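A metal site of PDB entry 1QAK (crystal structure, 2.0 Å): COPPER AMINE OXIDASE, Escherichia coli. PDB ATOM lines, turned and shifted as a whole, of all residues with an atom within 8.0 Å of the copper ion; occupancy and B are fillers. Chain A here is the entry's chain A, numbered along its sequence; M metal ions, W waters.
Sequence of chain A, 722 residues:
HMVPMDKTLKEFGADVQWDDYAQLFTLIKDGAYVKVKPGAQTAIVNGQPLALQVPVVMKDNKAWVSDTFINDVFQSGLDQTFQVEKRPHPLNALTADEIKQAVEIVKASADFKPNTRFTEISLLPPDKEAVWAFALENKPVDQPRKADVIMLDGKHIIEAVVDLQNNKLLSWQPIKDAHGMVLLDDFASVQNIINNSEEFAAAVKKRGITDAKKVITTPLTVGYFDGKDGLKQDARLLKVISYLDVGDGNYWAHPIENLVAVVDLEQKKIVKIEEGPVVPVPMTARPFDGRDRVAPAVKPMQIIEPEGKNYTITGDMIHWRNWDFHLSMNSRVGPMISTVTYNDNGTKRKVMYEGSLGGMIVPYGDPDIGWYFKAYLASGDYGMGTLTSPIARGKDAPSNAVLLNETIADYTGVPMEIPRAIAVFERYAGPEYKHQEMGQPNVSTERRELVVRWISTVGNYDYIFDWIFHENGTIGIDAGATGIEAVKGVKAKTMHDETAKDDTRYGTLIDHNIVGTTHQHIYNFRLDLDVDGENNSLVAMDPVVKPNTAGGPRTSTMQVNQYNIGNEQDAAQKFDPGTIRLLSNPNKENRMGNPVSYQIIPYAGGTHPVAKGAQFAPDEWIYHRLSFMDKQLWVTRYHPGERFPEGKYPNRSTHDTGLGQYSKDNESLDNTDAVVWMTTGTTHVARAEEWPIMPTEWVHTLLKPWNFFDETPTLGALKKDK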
ATOM      1  N   VAL A 362     -19.249   0.019   4.183  1.00  0.00           N
ATOM      2  CA  VAL A 362     -20.431  -0.280   3.380  1.00  0.00           C
ATOM      3  C   VAL A 362     -21.590   0.023   4.335  1.00  0.00           C
ATOM      4  O   VAL A 362     -22.086  -0.910   5.002  1.00  0.00           O
ATOM      5  CB  VAL A 362     -20.427  -1.759   2.938  1.00  0.00           C
ATOM      6  CG1 VAL A 362     -21.720  -2.130   2.213  1.00  0.00           C
ATOM      7  CG2 VAL A 362     -19.322  -2.106   1.958  1.00  0.00           C
ATOM      8  N   TYR A 364     -25.467   1.274   5.423  1.00  0.00           N
ATOM      9  CA  TYR A 364     -26.817   1.157   4.884  1.00  0.00           C
ATOM     10  C   TYR A 364     -27.761   2.328   5.067  1.00  0.00           C
ATOM     11  O   TYR A 364     -27.501   3.211   5.882  1.00  0.00           O
ATOM     12  CB  TYR A 364     -27.427  -0.137   5.485  1.00  0.00           C
ATOM     13  CG  TYR A 364     -26.808  -1.325   4.785  1.00  0.00           C
ATOM     14  CD1 TYR A 364     -25.554  -1.787   5.169  1.00  0.00           C
ATOM     15  CD2 TYR A 364     -27.455  -1.960   3.729  1.00  0.00           C
ATOM     16  CE1 TYR A 364     -24.971  -2.861   4.522  1.00  0.00           C
ATOM     17  CE2 TYR A 364     -26.880  -3.045   3.085  1.00  0.00           C
ATOM     18  CZ  TYR A 364     -25.629  -3.481   3.490  1.00  0.00           C
ATOM     19  OH  TYR A 364     -25.072  -4.562   2.823  1.00  0.00           O
ATOM     20  N   ASN A 460     -21.216 -11.424   3.964  1.00  0.00           N
ATOM     21  CA  ASN A 460     -21.766 -11.773   2.661  1.00  0.00           C
ATOM     22  C   ASN A 460     -21.095 -11.134   1.460  1.00  0.00           C
ATOM     23  O   ASN A 460     -21.306 -11.556   0.345  1.00  0.00           O
ATOM     24  CB  ASN A 460     -23.208 -11.217   2.634  1.00  0.00           C
ATOM     25  CG  ASN A 460     -23.271  -9.806   3.213  1.00  0.00           C
ATOM     26  OD1 ASN A 460     -22.776  -9.384   4.248  1.00  0.00           O
ATOM     27  ND2 ASN A 460     -23.939  -8.943   2.454  1.00  0.00           N
ATOM     28  N   TPQ A 461     -20.276 -10.131   1.704  1.00  0.00           N
ATOM     29  CA  TPQ A 461     -19.681  -9.507   0.527  1.00  0.00           C
ATOM     30  CB  TPQ A 461     -19.286  -7.992   0.422  1.00  0.00           C
ATOM     31  C   TPQ A 461     -18.199  -9.438   0.242  1.00  0.00           C
ATOM     32  O   TPQ A 461     -17.504 -10.116   1.043  1.00  0.00           O
ATOM     33  C1  TPQ A 461     -20.586  -7.273  -0.024  1.00  0.00           C
ATOM     34  C2  TPQ A 461     -21.524  -6.616   0.790  1.00  0.00           C
ATOM     35  O2  TPQ A 461     -21.366  -6.582   2.045  1.00  0.00           O
ATOM     36  C3  TPQ A 461     -22.701  -5.990   0.258  1.00  0.00           C
ATOM     37  C4  TPQ A 461     -22.873  -6.033  -1.112  1.00  0.00           C
ATOM     38  O4  TPQ A 461     -23.916  -5.505  -1.812  1.00  0.00           O
ATOM     39  C5  TPQ A 461     -21.889  -6.704  -1.908  1.00  0.00           C
ATOM     40  O5  TPQ A 461     -22.032  -6.767  -3.227  1.00  0.00           O
ATOM     41  C6  TPQ A 461     -20.805  -7.282  -1.347  1.00  0.00           C
ATOM     42  N   TYR A 463     -14.740  -8.565  -1.828  1.00  0.00           N
ATOM     43  CA  TYR A 463     -14.061  -7.391  -2.376  1.00  0.00           C
ATOM     44  C   TYR A 463     -12.783  -7.719  -3.086  1.00  0.00           C
ATOM     45  O   TYR A 463     -11.950  -8.440  -2.571  1.00  0.00           O
ATOM     46  CB  TYR A 463     -13.862  -6.386  -1.223  1.00  0.00           C
ATOM     47  CG  TYR A 463     -15.234  -5.897  -0.765  1.00  0.00           C
ATOM     48  CD1 TYR A 463     -15.997  -5.063  -1.588  1.00  0.00           C
ATOM     49  CD2 TYR A 463     -15.761  -6.302   0.453  1.00  0.00           C
ATOM     50  CE1 TYR A 463     -17.248  -4.606  -1.217  1.00  0.00           C
ATOM     51  CE2 TYR A 463     -17.019  -5.832   0.826  1.00  0.00           C
ATOM     52  CZ  TYR A 463     -17.752  -5.017   0.003  1.00  0.00           C
ATOM     53  OH  TYR A 463     -18.975  -4.650   0.502  1.00  0.00           O
ATOM     54  N   ALA A 481     -16.775  -5.435  -6.627  1.00  0.00           N
ATOM     55  CA  ALA A 481     -17.599  -5.935  -5.530  1.00  0.00           C
ATOM     56  C   ALA A 481     -18.492  -7.029  -6.056  1.00  0.00           C
ATOM     57  O   ALA A 481     -19.050  -6.912  -7.137  1.00  0.00           O
ATOM     58  CB  ALA A 481     -18.429  -4.777  -4.961  1.00  0.00           C
ATOM     59  N   THR A 482     -18.621  -8.116  -5.326  1.00  0.00           N
ATOM     60  CA  THR A 482     -19.462  -9.240  -5.735  1.00  0.00           C
ATOM     61  C   THR A 482     -19.898  -9.917  -4.439  1.00  0.00           C
ATOM     62  O   THR A 482     -19.630  -9.402  -3.353  1.00  0.00           O
ATOM     63  CB  THR A 482     -18.865 -10.166  -6.799  1.00  0.00           C
ATOM     64  OG1 THR A 482     -19.794 -11.215  -7.106  1.00  0.00           O
ATOM     65  CG2 THR A 482     -17.573 -10.898  -6.439  1.00  0.00           C
ATOM     66  N   ILE A 484     -23.112 -11.844  -2.021  1.00  0.00           N
ATOM     67  CA  ILE A 484     -24.534 -11.914  -1.758  1.00  0.00           C
ATOM     68  C   ILE A 484     -25.028 -10.644  -1.073  1.00  0.00           C
ATOM     69  O   ILE A 484     -24.499 -10.221  -0.047  1.00  0.00           O
ATOM     70  CB  ILE A 484     -24.728 -13.073  -0.716  1.00  0.00           C
ATOM     71  CG1 ILE A 484     -23.984 -14.376  -1.090  1.00  0.00           C
ATOM     72  CG2 ILE A 484     -26.237 -13.377  -0.669  1.00  0.00           C
ATOM     73  CD1 ILE A 484     -24.228 -14.832  -2.526  1.00  0.00           C
ATOM     74  N   GLU A 485     -26.063 -10.041  -1.650  1.00  0.00           N
ATOM     75  CA  GLU A 485     -26.564  -8.813  -1.006  1.00  0.00           C
ATOM     76  C   GLU A 485     -27.239  -9.088   0.341  1.00  0.00           C
ATOM     77  O   GLU A 485     -27.774 -10.150   0.591  1.00  0.00           O
ATOM     78  CB  GLU A 485     -27.652  -8.252  -1.946  1.00  0.00           C
ATOM     79  CG  GLU A 485     -26.987  -7.470  -3.083  1.00  0.00           C
ATOM     80  CD  GLU A 485     -28.003  -6.848  -4.013  1.00  0.00           C
ATOM     81  OE1 GLU A 485     -29.143  -6.519  -3.615  1.00  0.00           O
ATOM     82  OE2 GLU A 485     -27.648  -6.657  -5.211  1.00  0.00           O
ATOM     83  N   ALA A 486     -27.192  -8.135   1.241  1.00  0.00           N
ATOM     84  CA  ALA A 486     -27.780  -8.158   2.581  1.00  0.00           C
ATOM     85  C   ALA A 486     -29.242  -7.791   2.256  1.00  0.00           C
ATOM     86  O   ALA A 486     -29.456  -6.682   1.728  1.00  0.00           O
ATOM     87  CB  ALA A 486     -27.056  -7.036   3.312  1.00  0.00           C
ATOM     88  N   THR A 517     -31.612  -3.772   0.456  1.00  0.00           N
ATOM     89  CA  THR A 517     -31.555  -2.453   1.058  1.00  0.00           C
ATOM     90  C   THR A 517     -30.440  -1.615   0.450  1.00  0.00           C
ATOM     91  O   THR A 517     -29.288  -2.064   0.303  1.00  0.00           O
ATOM     92  CB  THR A 517     -31.329  -2.623   2.566  1.00  0.00           C
ATOM     93  OG1 THR A 517     -32.399  -3.470   3.038  1.00  0.00           O
ATOM     94  CG2 THR A 517     -31.291  -1.282   3.259  1.00  0.00           C
ATOM     95  N   THR A 518     -30.841  -0.375   0.120  1.00  0.00           N
ATOM     96  CA  THR A 518     -29.865   0.554  -0.470  1.00  0.00           C
ATOM     97  C   THR A 518     -28.694   0.811   0.454  1.00  0.00           C
ATOM     98  O   THR A 518     -28.848   0.878   1.668  1.00  0.00           O
ATOM     99  CB  THR A 518     -30.523   1.897  -0.868  1.00  0.00           C
ATOM    100  OG1 THR A 518     -31.478   1.576  -1.903  1.00  0.00           O
ATOM    101  CG2 THR A 518     -29.545   2.876  -1.511  1.00  0.00           C
ATOM    102  N   HIS A 519     -27.497   0.954  -0.108  1.00  0.00           N
ATOM    103  CA  HIS A 519     -26.338   1.224   0.751  1.00  0.00           C
ATOM    104  C   HIS A 519     -25.245   1.782  -0.178  1.00  0.00           C
ATOM    105  O   HIS A 519     -25.492   1.821  -1.368  1.00  0.00           O
ATOM    106  CB  HIS A 519     -25.890  -0.081   1.417  1.00  0.00           C
ATOM    107  CG  HIS A 519     -25.646  -1.120   0.366  1.00  0.00           C
ATOM    108  ND1 HIS A 519     -26.667  -1.858  -0.229  1.00  0.00           N
ATOM    109  CD2 HIS A 519     -24.472  -1.488  -0.206  1.00  0.00           C
ATOM    110  CE1 HIS A 519     -26.157  -2.689  -1.128  1.00  0.00           C
ATOM    111  NE2 HIS A 519     -24.866  -2.444  -1.080  1.00  0.00           N
ATOM    112  N   GLN A 520     -24.104   2.177   0.350  1.00  0.00           N
ATOM    113  CA  GLN A 520     -23.024   2.696  -0.451  1.00  0.00           C
ATOM    114  C   GLN A 520     -21.835   1.768  -0.211  1.00  0.00           C
ATOM    115  O   GLN A 520     -21.782   1.056   0.796  1.00  0.00           O
ATOM    116  CB  GLN A 520     -22.599   4.017   0.222  1.00  0.00           C
ATOM    117  CG  GLN A 520     -23.617   5.126  -0.120  1.00  0.00           C
ATOM    118  CD  GLN A 520     -23.072   6.498   0.142  1.00  0.00           C
ATOM    119  OE1 GLN A 520     -22.708   7.108  -0.872  1.00  0.00           O
ATOM    120  NE2 GLN A 520     -23.018   7.004   1.359  1.00  0.00           N
ATOM    121  N   HIS A 521     -20.883   1.787  -1.115  1.00  0.00           N
ATOM    122  CA  HIS A 521     -19.639   0.996  -1.017  1.00  0.00           C
ATOM    123  C   HIS A 521     -18.634   2.166  -1.060  1.00  0.00           C
ATOM    124  O   HIS A 521     -18.587   2.877  -2.069  1.00  0.00           O
ATOM    125  CB  HIS A 521     -19.321   0.105  -2.221  1.00  0.00           C
ATOM    126  CG  HIS A 521     -20.198  -1.088  -2.218  1.00  0.00           C
ATOM    127  ND1 HIS A 521     -19.783  -2.290  -1.679  1.00  0.00           N
ATOM    128  CD2 HIS A 521     -21.454  -1.264  -2.678  1.00  0.00           C
ATOM    129  CE1 HIS A 521     -20.720  -3.225  -1.768  1.00  0.00           C
ATOM    130  NE2 HIS A 521     -21.680  -2.575  -2.375  1.00  0.00           N
ATOM    131  N   TYR A 523     -14.638   3.095  -0.697  1.00  0.00           N
ATOM    132  CA  TYR A 523     -13.274   2.628  -0.534  1.00  0.00           C
ATOM    133  C   TYR A 523     -12.342   3.852  -0.404  1.00  0.00           C
ATOM    134  O   TYR A 523     -12.563   4.877  -1.086  1.00  0.00           O
ATOM    135  CB  TYR A 523     -12.775   1.867  -1.791  1.00  0.00           C
ATOM    136  CG  TYR A 523     -13.772   0.858  -2.303  1.00  0.00           C
ATOM    137  CD1 TYR A 523     -13.771  -0.432  -1.781  1.00  0.00           C
ATOM    138  CD2 TYR A 523     -14.716   1.137  -3.285  1.00  0.00           C
ATOM    139  CE1 TYR A 523     -14.677  -1.385  -2.208  1.00  0.00           C
ATOM    140  CE2 TYR A 523     -15.635   0.196  -3.725  1.00  0.00           C
ATOM    141  CZ  TYR A 523     -15.594  -1.073  -3.172  1.00  0.00           C
ATOM    142  OH  TYR A 523     -16.484  -2.066  -3.555  1.00  0.00           O
ATOM    143  N   HIS A 608     -21.623   0.937 -11.198  1.00  0.00           N
ATOM    144  CA  HIS A 608     -22.816   1.112 -10.397  1.00  0.00           C
ATOM    145  C   HIS A 608     -22.887   2.645 -10.281  1.00  0.00           C
ATOM    146  O   HIS A 608     -21.927   3.354 -10.611  1.00  0.00           O
ATOM    147  CB  HIS A 608     -22.679   0.667  -8.931  1.00  0.00           C
ATOM    148  CG  HIS A 608     -23.365  -0.642  -8.645  1.00  0.00           C
ATOM    149  ND1 HIS A 608     -23.019  -1.400  -7.537  1.00  0.00           N
ATOM    150  CD2 HIS A 608     -24.323  -1.297  -9.322  1.00  0.00           C
ATOM    151  CE1 HIS A 608     -23.777  -2.486  -7.565  1.00  0.00           C
ATOM    152  NE2 HIS A 608     -24.565  -2.458  -8.640  1.00  0.00           N
ATOM    153  N   THR A 682     -19.736   4.047  -4.285  1.00  0.00           N
ATOM    154  CA  THR A 682     -20.858   3.813  -5.174  1.00  0.00           C
ATOM    155  C   THR A 682     -22.129   3.906  -4.323  1.00  0.00           C
ATOM    156  O   THR A 682     -21.989   3.693  -3.130  1.00  0.00           O
ATOM    157  CB  THR A 682     -20.914   2.374  -5.717  1.00  0.00           C
ATOM    158  OG1 THR A 682     -21.137   1.453  -4.629  1.00  0.00           O
ATOM    159  CG2 THR A 682     -19.684   1.992  -6.505  1.00  0.00           C
ATOM    160  N   THR A 683     -23.262   4.156  -4.963  1.00  0.00           N
ATOM    161  CA  THR A 683     -24.499   4.185  -4.196  1.00  0.00           C
ATOM    162  C   THR A 683     -25.183   2.982  -4.860  1.00  0.00           C
ATOM    163  O   THR A 683     -25.450   3.079  -6.068  1.00  0.00           O
ATOM    164  CB  THR A 683     -25.283   5.494  -4.421  1.00  0.00           C
ATOM    165  OG1 THR A 683     -24.535   6.398  -3.601  1.00  0.00           O
ATOM    166  CG2 THR A 683     -26.674   5.236  -3.869  1.00  0.00           C
ATOM    167  N   HIS A 684     -25.402   1.923  -4.077  1.00  0.00           N
ATOM    168  CA  HIS A 684     -26.016   0.767  -4.698  1.00  0.00           C
ATOM    169  C   HIS A 684     -27.519   0.612  -4.510  1.00  0.00           C
ATOM    170  O   HIS A 684     -27.972   0.319  -3.424  1.00  0.00           O
ATOM    171  CB  HIS A 684     -25.350  -0.543  -4.203  1.00  0.00           C
ATOM    172  CG  HIS A 684     -25.783  -1.847  -4.777  1.00  0.00           C
ATOM    173  ND1 HIS A 684     -25.267  -3.058  -4.373  1.00  0.00           N
ATOM    174  CD2 HIS A 684     -26.712  -2.184  -5.703  1.00  0.00           C
ATOM    175  CE1 HIS A 684     -25.798  -4.088  -5.004  1.00  0.00           C
ATOM    176  NE2 HIS A 684     -26.702  -3.562  -5.825  1.00  0.00           N
ATOM    177  N   VAL A 685     -28.255   0.813  -5.587  1.00  0.00           N
ATOM    178  CA  VAL A 685     -29.715   0.655  -5.578  1.00  0.00           C
ATOM    179  C   VAL A 685     -29.800  -0.685  -6.306  1.00  0.00           C
ATOM    180  O   VAL A 685     -29.403  -0.789  -7.460  1.00  0.00           O
ATOM    181  CB  VAL A 685     -30.544   1.760  -6.204  1.00  0.00           C
ATOM    182  CG1 VAL A 685     -32.020   1.361  -6.373  1.00  0.00           C
ATOM    183  CG2 VAL A 685     -30.366   3.039  -5.434  1.00  0.00           C
ATOM    184  N   ALA A 686     -30.272  -1.744  -5.666  1.00  0.00           N
ATOM    185  CA  ALA A 686     -30.365  -3.079  -6.225  1.00  0.00           C
ATOM    186  C   ALA A 686     -31.325  -3.395  -7.340  1.00  0.00           C
ATOM    187  O   ALA A 686     -32.239  -2.656  -7.678  1.00  0.00           O
ATOM    188  CB  ALA A 686     -30.682  -4.087  -5.104  1.00  0.00           C
ATOM    189  N   GLU A 690     -29.120  -8.997  -9.642  1.00  0.00           N
ATOM    190  CA  GLU A 690     -28.092  -9.185  -8.611  1.00  0.00           C
ATOM    191  C   GLU A 690     -28.430 -10.194  -7.538  1.00  0.00           C
ATOM    192  O   GLU A 690     -27.696 -10.306  -6.564  1.00  0.00           O
ATOM    193  CB  GLU A 690     -27.778  -7.814  -7.970  1.00  0.00           C
ATOM    194  CG  GLU A 690     -27.353  -6.754  -8.983  1.00  0.00           C
ATOM    195  CD  GLU A 690     -27.409  -5.329  -8.458  1.00  0.00           C
ATOM    196  OE1 GLU A 690     -27.999  -5.050  -7.397  1.00  0.00           O
ATOM    197  OE2 GLU A 690     -26.825  -4.439  -9.146  1.00  0.00           O
ATOM    198  N   MET A 694     -24.444 -11.439  -6.826  1.00  0.00           N
ATOM    199  CA  MET A 694     -24.233 -10.237  -7.635  1.00  0.00           C
ATOM    200  C   MET A 694     -23.062 -10.235  -8.601  1.00  0.00           C
ATOM    201  O   MET A 694     -21.916 -10.400  -8.217  1.00  0.00           O
ATOM    202  CB  MET A 694     -23.938  -9.024  -6.734  1.00  0.00           C
ATOM    203  CG  MET A 694     -23.823  -7.746  -7.595  1.00  0.00           C
ATOM    204  SD  MET A 694     -23.780  -6.216  -6.635  1.00  0.00           S
ATOM    205  CE  MET A 694     -22.000  -6.132  -6.326  1.00  0.00           C
ATOM    206  N   GLU A 697     -19.203  -5.761  -9.951  1.00  0.00           N
ATOM    207  CA  GLU A 697     -19.348  -4.347 -10.263  1.00  0.00           C
ATOM    208  C   GLU A 697     -17.983  -3.716  -9.920  1.00  0.00           C
ATOM    209  O   GLU A 697     -17.346  -4.053  -8.897  1.00  0.00           O
ATOM    210  CB  GLU A 697     -20.456  -3.669  -9.467  1.00  0.00           C
ATOM    211  CG  GLU A 697     -21.816  -4.327  -9.780  1.00  0.00           C
ATOM    212  CD  GLU A 697     -22.510  -3.812 -11.009  1.00  0.00           C
ATOM    213  OE1 GLU A 697     -21.871  -3.061 -11.790  1.00  0.00           O
ATOM    214  OE2 GLU A 697     -23.715  -4.188 -11.203  1.00  0.00           O
HETATM  215 CU    CU M   1     -23.654  -3.191  -2.826  1.00  0.00          CU
HETATM  216  O   HOH W   1     -21.428  -3.943  -4.555  1.00  0.00           O
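The copper ion is bound by a ring nitrogen (NE2) of His 521 (2.1 Å), a ring nitrogen (ND1) of His 684 (2.2 Å), a ring nitrogen (NE2) of His 519 (2.3 Å) and O4 of TPQ 461 (2.5 Å).
The nearest printed residue that does not touch the copper ion is His 608 (4.8 Å).
The backbone carbonyl oxygen of His 521 sits at hydrogen-bond distance from the backbone NH of Thr 682 (2.8 Å). ND1 of His 521 lies close to OH of Tyr 463 (3.3 Å). The side-chain carboxylate of Glu 485 lies close to a ring nitrogen (NE2) of His 684 (3.3 Å). NE2 of His 684 lies within hydrogen-bond range of OE1 of Glu 690 (2.5 Å). The backbone carbonyl oxygen (O) of Thr 517 sits at hydrogen-bond distance from a ring nitrogen (ND1) of His 519 (2.7 Å). O2 of TPQ 461 lies close to OH of Tyr 463 (3.4 Å).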
